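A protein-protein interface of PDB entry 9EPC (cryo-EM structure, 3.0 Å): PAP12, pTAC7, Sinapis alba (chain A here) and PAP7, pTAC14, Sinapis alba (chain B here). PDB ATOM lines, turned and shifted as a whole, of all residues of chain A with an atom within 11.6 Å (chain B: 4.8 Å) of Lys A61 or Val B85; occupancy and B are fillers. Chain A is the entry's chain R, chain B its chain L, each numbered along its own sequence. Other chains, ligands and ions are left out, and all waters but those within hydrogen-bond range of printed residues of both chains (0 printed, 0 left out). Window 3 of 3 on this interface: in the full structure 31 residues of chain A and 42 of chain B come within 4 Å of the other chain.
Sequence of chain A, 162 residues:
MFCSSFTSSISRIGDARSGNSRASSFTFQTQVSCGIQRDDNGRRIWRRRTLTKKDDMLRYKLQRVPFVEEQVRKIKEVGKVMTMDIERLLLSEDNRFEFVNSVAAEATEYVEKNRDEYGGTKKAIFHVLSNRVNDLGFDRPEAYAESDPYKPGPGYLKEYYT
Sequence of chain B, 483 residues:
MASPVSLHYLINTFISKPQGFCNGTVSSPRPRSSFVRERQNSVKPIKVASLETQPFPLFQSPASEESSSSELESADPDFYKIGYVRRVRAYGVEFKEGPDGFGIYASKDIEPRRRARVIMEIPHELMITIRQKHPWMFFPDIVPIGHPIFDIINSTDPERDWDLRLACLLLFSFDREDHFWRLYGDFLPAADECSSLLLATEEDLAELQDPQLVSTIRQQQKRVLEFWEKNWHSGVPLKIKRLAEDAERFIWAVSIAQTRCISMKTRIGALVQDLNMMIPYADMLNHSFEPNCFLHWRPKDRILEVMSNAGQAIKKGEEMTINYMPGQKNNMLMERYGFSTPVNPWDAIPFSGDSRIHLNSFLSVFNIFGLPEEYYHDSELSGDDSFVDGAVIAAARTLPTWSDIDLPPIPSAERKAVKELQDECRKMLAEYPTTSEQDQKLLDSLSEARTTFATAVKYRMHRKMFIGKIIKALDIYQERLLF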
ATOM      1  N   LEU A  51      22.937 -11.168  33.995  1.00  0.00           N
ATOM      2  CA  LEU A  51      21.644 -10.503  33.852  1.00  0.00           C
ATOM      3  C   LEU A  51      20.691 -11.048  34.908  1.00  0.00           C
ATOM      4  O   LEU A  51      20.197 -12.172  34.799  1.00  0.00           O
ATOM      5  CB  LEU A  51      21.095 -10.721  32.447  1.00  0.00           C
ATOM      6  CG  LEU A  51      19.783 -10.017  32.107  1.00  0.00           C
ATOM      7  CD1 LEU A  51      19.948  -8.509  32.191  1.00  0.00           C
ATOM      8  CD2 LEU A  51      19.306 -10.432  30.728  1.00  0.00           C
ATOM      9  N   LYS A  54      14.956 -10.702  33.530  1.00  0.00           N
ATOM     10  CA  LYS A  54      14.720 -11.467  32.315  1.00  0.00           C
ATOM     11  C   LYS A  54      14.297 -10.540  31.185  1.00  0.00           C
ATOM     12  O   LYS A  54      13.488  -9.630  31.384  1.00  0.00           O
ATOM     13  CB  LYS A  54      13.654 -12.544  32.542  1.00  0.00           C
ATOM     14  CG  LYS A  54      13.371 -13.401  31.321  1.00  0.00           C
ATOM     15  CD  LYS A  54      14.647 -14.015  30.767  1.00  0.00           C
ATOM     16  CE  LYS A  54      14.388 -14.732  29.453  1.00  0.00           C
ATOM     17  NZ  LYS A  54      15.638 -15.282  28.862  1.00  0.00           N
ATOM     18  N   ASP A  55      14.848 -10.784  29.997  1.00  0.00           N
ATOM     19  CA  ASP A  55      14.562  -9.987  28.812  1.00  0.00           C
ATOM     20  C   ASP A  55      13.535 -10.718  27.957  1.00  0.00           C
ATOM     21  O   ASP A  55      13.774 -11.851  27.524  1.00  0.00           O
ATOM     22  CB  ASP A  55      15.841  -9.719  28.019  1.00  0.00           C
ATOM     23  CG  ASP A  55      15.582  -9.003  26.704  1.00  0.00           C
ATOM     24  OD1 ASP A  55      15.071  -9.639  25.761  1.00  0.00           O
ATOM     25  OD2 ASP A  55      15.887  -7.798  26.610  1.00  0.00           O
ATOM     26  N   ASP A  56      12.396 -10.065  27.716  1.00  0.00           N
ATOM     27  CA  ASP A  56      11.346 -10.672  26.905  1.00  0.00           C
ATOM     28  C   ASP A  56      11.804 -10.881  25.468  1.00  0.00           C
ATOM     29  O   ASP A  56      11.583 -11.948  24.885  1.00  0.00           O
ATOM     30  CB  ASP A  56      10.099  -9.790  26.937  1.00  0.00           C
ATOM     31  CG  ASP A  56       9.681  -9.430  28.345  1.00  0.00           C
ATOM     32  OD1 ASP A  56       8.608  -9.892  28.785  1.00  0.00           O
ATOM     33  OD2 ASP A  56      10.438  -8.702  29.020  1.00  0.00           O
ATOM     34  N   MET A  57      12.455  -9.873  24.885  1.00  0.00           N
ATOM     35  CA  MET A  57      12.844  -9.931  23.483  1.00  0.00           C
ATOM     36  C   MET A  57      13.933 -10.964  23.225  1.00  0.00           C
ATOM     37  O   MET A  57      14.141 -11.355  22.072  1.00  0.00           O
ATOM     38  CB  MET A  57      13.300  -8.542  23.030  1.00  0.00           C
ATOM     39  CG  MET A  57      13.285  -8.312  21.529  1.00  0.00           C
ATOM     40  SD  MET A  57      13.822  -6.650  21.077  1.00  0.00           S
ATOM     41  CE  MET A  57      13.503  -5.754  22.594  1.00  0.00           C
ATOM     42  N   LEU A  58      14.621 -11.421  24.274  1.00  0.00           N
ATOM     43  CA  LEU A  58      15.696 -12.390  24.091  1.00  0.00           C
ATOM     44  C   LEU A  58      15.174 -13.701  23.518  1.00  0.00           C
ATOM     45  O   LEU A  58      15.786 -14.280  22.613  1.00  0.00           O
ATOM     46  CB  LEU A  58      16.408 -12.631  25.420  1.00  0.00           C
ATOM     47  CG  LEU A  58      17.900 -12.308  25.422  1.00  0.00           C
ATOM     48  CD1 LEU A  58      18.509 -12.583  26.785  1.00  0.00           C
ATOM     49  CD2 LEU A  58      18.601 -13.110  24.346  1.00  0.00           C
ATOM     50  N   ARG A  59      14.039 -14.183  24.026  1.00  0.00           N
ATOM     51  CA  ARG A  59      13.476 -15.435  23.539  1.00  0.00           C
ATOM     52  C   ARG A  59      12.708 -15.266  22.237  1.00  0.00           C
ATOM     53  O   ARG A  59      12.415 -16.266  21.572  1.00  0.00           O
ATOM     54  CB  ARG A  59      12.555 -16.042  24.600  1.00  0.00           C
ATOM     55  CG  ARG A  59      11.292 -15.238  24.837  1.00  0.00           C
ATOM     56  CD  ARG A  59      10.417 -15.866  25.907  1.00  0.00           C
ATOM     57  NE  ARG A  59      10.899 -15.568  27.249  1.00  0.00           N
ATOM     58  CZ  ARG A  59      10.521 -14.515  27.961  1.00  0.00           C
ATOM     59  NH1 ARG A  59       9.655 -13.635  27.487  1.00  0.00           N
ATOM     60  NH2 ARG A  59      11.024 -14.342  29.180  1.00  0.00           N
ATOM     61  N   TYR A  60      12.379 -14.035  21.857  1.00  0.00           N
ATOM     62  CA  TYR A  60      11.567 -13.766  20.678  1.00  0.00           C
ATOM     63  C   TYR A  60      12.389 -13.424  19.442  1.00  0.00           C
ATOM     64  O   TYR A  60      11.804 -13.143  18.392  1.00  0.00           O
ATOM     65  CB  TYR A  60      10.586 -12.624  20.964  1.00  0.00           C
ATOM     66  CG  TYR A  60       9.593 -12.915  22.066  1.00  0.00           C
ATOM     67  CD1 TYR A  60       9.151 -14.209  22.305  1.00  0.00           C
ATOM     68  CD2 TYR A  60       9.096 -11.895  22.865  1.00  0.00           C
ATOM     69  CE1 TYR A  60       8.243 -14.479  23.312  1.00  0.00           C
ATOM     70  CE2 TYR A  60       8.189 -12.155  23.874  1.00  0.00           C
ATOM     71  CZ  TYR A  60       7.766 -13.447  24.093  1.00  0.00           C
ATOM     72  OH  TYR A  60       6.862 -13.712  25.095  1.00  0.00           O
ATOM     73  N   LYS A  61      13.721 -13.438  19.531  1.00  0.00           N
ATOM     74  CA  LYS A  61      14.552 -13.005  18.416  1.00  0.00           C
ATOM     75  C   LYS A  61      15.713 -13.929  18.076  1.00  0.00           C
ATOM     76  O   LYS A  61      16.360 -13.706  17.049  1.00  0.00           O
ATOM     77  CB  LYS A  61      15.116 -11.600  18.679  1.00  0.00           C
ATOM     78  CG  LYS A  61      14.212 -10.470  18.221  1.00  0.00           C
ATOM     79  CD  LYS A  61      14.943  -9.141  18.279  1.00  0.00           C
ATOM     80  CE  LYS A  61      14.135  -8.030  17.639  1.00  0.00           C
ATOM     81  NZ  LYS A  61      13.870  -8.303  16.202  1.00  0.00           N
ATOM     82  N   LEU A  62      16.001 -14.946  18.885  1.00  0.00           N
ATOM     83  CA  LEU A  62      17.136 -15.811  18.591  1.00  0.00           C
ATOM     84  C   LEU A  62      16.829 -16.857  17.528  1.00  0.00           C
ATOM     85  O   LEU A  62      17.759 -17.507  17.040  1.00  0.00           O
ATOM     86  CB  LEU A  62      17.628 -16.504  19.866  1.00  0.00           C
ATOM     87  CG  LEU A  62      16.832 -17.687  20.424  1.00  0.00           C
ATOM     88  CD1 LEU A  62      17.707 -18.515  21.349  1.00  0.00           C
ATOM     89  CD2 LEU A  62      15.594 -17.216  21.163  1.00  0.00           C
ATOM     90  N   GLN A  63      15.564 -17.034  17.156  1.00  0.00           N
ATOM     91  CA  GLN A  63      15.206 -18.023  16.150  1.00  0.00           C
ATOM     92  C   GLN A  63      15.546 -17.529  14.749  1.00  0.00           C
ATOM     93  O   GLN A  63      15.539 -16.327  14.468  1.00  0.00           O
ATOM     94  CB  GLN A  63      13.716 -18.362  16.228  1.00  0.00           C
ATOM     95  CG  GLN A  63      13.341 -19.287  17.375  1.00  0.00           C
ATOM     96  CD  GLN A  63      13.390 -18.601  18.723  1.00  0.00           C
ATOM     97  OE1 GLN A  63      13.381 -17.372  18.808  1.00  0.00           O
ATOM     98  NE2 GLN A  63      13.443 -19.391  19.788  1.00  0.00           N
ATOM     99  N   ARG A  64      15.846 -18.478  13.867  1.00  0.00           N
ATOM    100  CA  ARG A  64      16.167 -18.201  12.474  1.00  0.00           C
ATOM    101  C   ARG A  64      15.278 -19.044  11.574  1.00  0.00           C
ATOM    102  O   ARG A  64      15.049 -20.227  11.848  1.00  0.00           O
ATOM    103  CB  ARG A  64      17.643 -18.489  12.177  1.00  0.00           C
ATOM    104  CG  ARG A  64      18.141 -19.804  12.753  1.00  0.00           C
ATOM    105  CD  ARG A  64      19.573 -20.101  12.335  1.00  0.00           C
ATOM    106  NE  ARG A  64      19.669 -20.476  10.929  1.00  0.00           N
ATOM    107  CZ  ARG A  64      20.026 -19.651   9.955  1.00  0.00           C
ATOM    108  NH1 ARG A  64      20.336 -18.388  10.198  1.00  0.00           N
ATOM    109  NH2 ARG A  64      20.078 -20.107   8.707  1.00  0.00           N
ATOM    110  N   VAL A  65      14.774 -18.433  10.506  1.00  0.00           N
ATOM    111  CA  VAL A  65      13.892 -19.126   9.572  1.00  0.00           C
ATOM    112  C   VAL A  65      14.701 -20.180   8.823  1.00  0.00           C
ATOM    113  O   VAL A  65      15.895 -19.976   8.556  1.00  0.00           O
ATOM    114  CB  VAL A  65      13.211 -18.144   8.607  1.00  0.00           C
ATOM    115  CG1 VAL A  65      12.463 -17.072   9.386  1.00  0.00           C
ATOM    116  CG2 VAL A  65      14.231 -17.521   7.681  1.00  0.00           C
ATOM    117  N   LYS B  81      23.863 -10.657  23.919  1.00  0.00           N
ATOM    118  CA  LYS B  81      22.568 -10.982  23.331  1.00  0.00           C
ATOM    119  C   LYS B  81      21.546  -9.876  23.561  1.00  0.00           C
ATOM    120  O   LYS B  81      20.799  -9.521  22.644  1.00  0.00           O
ATOM    121  CB  LYS B  81      22.059 -12.310  23.888  1.00  0.00           C
ATOM    122  CG  LYS B  81      22.702 -13.529  23.253  1.00  0.00           C
ATOM    123  CD  LYS B  81      22.229 -14.813  23.913  1.00  0.00           C
ATOM    124  CE  LYS B  81      22.930 -16.024  23.321  1.00  0.00           C
ATOM    125  NZ  LYS B  81      22.554 -17.279  24.023  1.00  0.00           N
ATOM    126  N   ILE B  82      21.494  -9.317  24.774  1.00  0.00           N
ATOM    127  CA  ILE B  82      20.523  -8.264  25.047  1.00  0.00           C
ATOM    128  C   ILE B  82      20.799  -7.029  24.211  1.00  0.00           C
ATOM    129  O   ILE B  82      19.892  -6.227  23.975  1.00  0.00           O
ATOM    130  CB  ILE B  82      20.485  -7.899  26.545  1.00  0.00           C
ATOM    131  CG1 ILE B  82      21.827  -7.330  27.001  1.00  0.00           C
ATOM    132  CG2 ILE B  82      20.076  -9.101  27.377  1.00  0.00           C
ATOM    133  CD1 ILE B  82      21.801  -6.769  28.403  1.00  0.00           C
ATOM    134  N   GLY B  83      22.037  -6.845  23.764  1.00  0.00           N
ATOM    135  CA  GLY B  83      22.349  -5.766  22.853  1.00  0.00           C
ATOM    136  C   GLY B  83      22.165  -6.189  21.413  1.00  0.00           C
ATOM    137  O   GLY B  83      21.734  -5.392  20.575  1.00  0.00           O
ATOM    138  N   TYR B  84      22.470  -7.456  21.122  1.00  0.00           N
ATOM    139  CA  TYR B  84      22.378  -7.945  19.751  1.00  0.00           C
ATOM    140  C   TYR B  84      20.959  -7.827  19.217  1.00  0.00           C
ATOM    141  O   TYR B  84      20.755  -7.497  18.042  1.00  0.00           O
ATOM    142  CB  TYR B  84      22.858  -9.394  19.676  1.00  0.00           C
ATOM    143  CG  TYR B  84      22.914  -9.944  18.272  1.00  0.00           C
ATOM    144  CD1 TYR B  84      24.027  -9.740  17.472  1.00  0.00           C
ATOM    145  CD2 TYR B  84      21.855 -10.671  17.748  1.00  0.00           C
ATOM    146  CE1 TYR B  84      24.084 -10.238  16.188  1.00  0.00           C
ATOM    147  CE2 TYR B  84      21.903 -11.173  16.465  1.00  0.00           C
ATOM    148  CZ  TYR B  84      23.019 -10.955  15.690  1.00  0.00           C
ATOM    149  OH  TYR B  84      23.072 -11.455  14.410  1.00  0.00           O
ATOM    150  N   VAL B  85      19.962  -8.094  20.063  1.00  0.00           N
ATOM    151  CA  VAL B  85      18.577  -7.940  19.644  1.00  0.00           C
ATOM    152  C   VAL B  85      18.227  -6.482  19.379  1.00  0.00           C
ATOM    153  O   VAL B  85      17.253  -6.202  18.673  1.00  0.00           O
ATOM    154  CB  VAL B  85      17.630  -8.545  20.695  1.00  0.00           C
ATOM    155  CG1 VAL B  85      17.873 -10.036  20.824  1.00  0.00           C
ATOM    156  CG2 VAL B  85      17.818  -7.862  22.033  1.00  0.00           C
ATOM    157  N   ARG B  86      18.997  -5.540  19.926  1.00  0.00           N
ATOM    158  CA  ARG B  86      18.774  -4.117  19.705  1.00  0.00           C
ATOM    159  C   ARG B  86      19.663  -3.558  18.603  1.00  0.00           C
ATOM    160  O   ARG B  86      20.026  -2.378  18.645  1.00  0.00           O
ATOM    161  CB  ARG B  86      18.995  -3.331  20.995  1.00  0.00           C
ATOM    162  CG  ARG B  86      18.553  -4.039  22.252  1.00  0.00           C
ATOM    163  CD  ARG B  86      17.062  -4.259  22.285  1.00  0.00           C
ATOM    164  NE  ARG B  86      16.681  -5.060  23.440  1.00  0.00           N
ATOM    165  CZ  ARG B  86      16.308  -4.560  24.609  1.00  0.00           C
ATOM    166  NH1 ARG B  86      16.238  -3.254  24.809  1.00  0.00           N
ATOM    167  NH2 ARG B  86      15.998  -5.388  25.601  1.00  0.00           N
ATOM    168  N   ARG B  87      20.033  -4.388  17.627  1.00  0.00           N
ATOM    169  CA  ARG B  87      20.839  -3.959  16.482  1.00  0.00           C
ATOM    170  C   ARG B  87      22.222  -3.477  16.927  1.00  0.00           C
ATOM    171  O   ARG B  87      22.738  -2.466  16.449  1.00  0.00           O
ATOM    172  CB  ARG B  87      20.100  -2.889  15.668  1.00  0.00           C
ATOM    173  CG  ARG B  87      20.691  -2.560  14.302  1.00  0.00           C
ATOM    174  CD  ARG B  87      21.235  -3.784  13.590  1.00  0.00           C
ATOM    175  NE  ARG B  87      21.832  -3.429  12.307  1.00  0.00           N
ATOM    176  CZ  ARG B  87      23.032  -2.884  12.165  1.00  0.00           C
ATOM    177  NH1 ARG B  87      23.798  -2.615  13.209  1.00  0.00           N
ATOM    178  NH2 ARG B  87      23.474  -2.597  10.944  1.00  0.00           N
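Hydrophobic or aromatic side chains of chain A that line the printed part of chain B: Leu A51, Met A57 and Leu A58.
Hydrophobic or aromatic side chains of chain B that line the printed part of chain A: Ile B82 and Val B85.
Among the printed residues, 6 pairs touch across the chains.
Ile B82 touches Leu A51 (CG2 to CD2, 3.7 Å).
Met A57 touches Arg B86.
Leu A58 touches Lys B81 (CD2 to CB, 3.6 Å).
CD1 of Leu A58 touches CG2 of Ile B82 (3.9 Å).
CD of Lys A61 touches CB of Val B85, at 3.7 Å.
Of the printed residues of chain B, Asp A55 touches Arg B86 (2.6 Å).
Asp A56 touches none of the printed residues of chain B.
Of the printed residues of chain B, Met A57 touches Arg B86.
Arg A64 touches none of the printed residues of chain B.
No residue of chain A comes within 4 Å of Gly B83.
Of chain A, only Lys A61 comes within 4 Å of Val B85.
Arg B86 touches just these residues of chain A: Asp A55 (2.6 Å) and Met A57 (3.4 Å).
OD2 of Asp A55 is in salt-bridge range of NH2 of Arg B86 (2.6 Å).
The guanidinium group (NE) of Arg B86 lies close to the backbone carbonyl oxygen (O) of Ile B82, 3.5 Å away.
OD1 of Asp A55 sits at hydrogen-bond distance from N of Met A57, at 2.8 Å.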
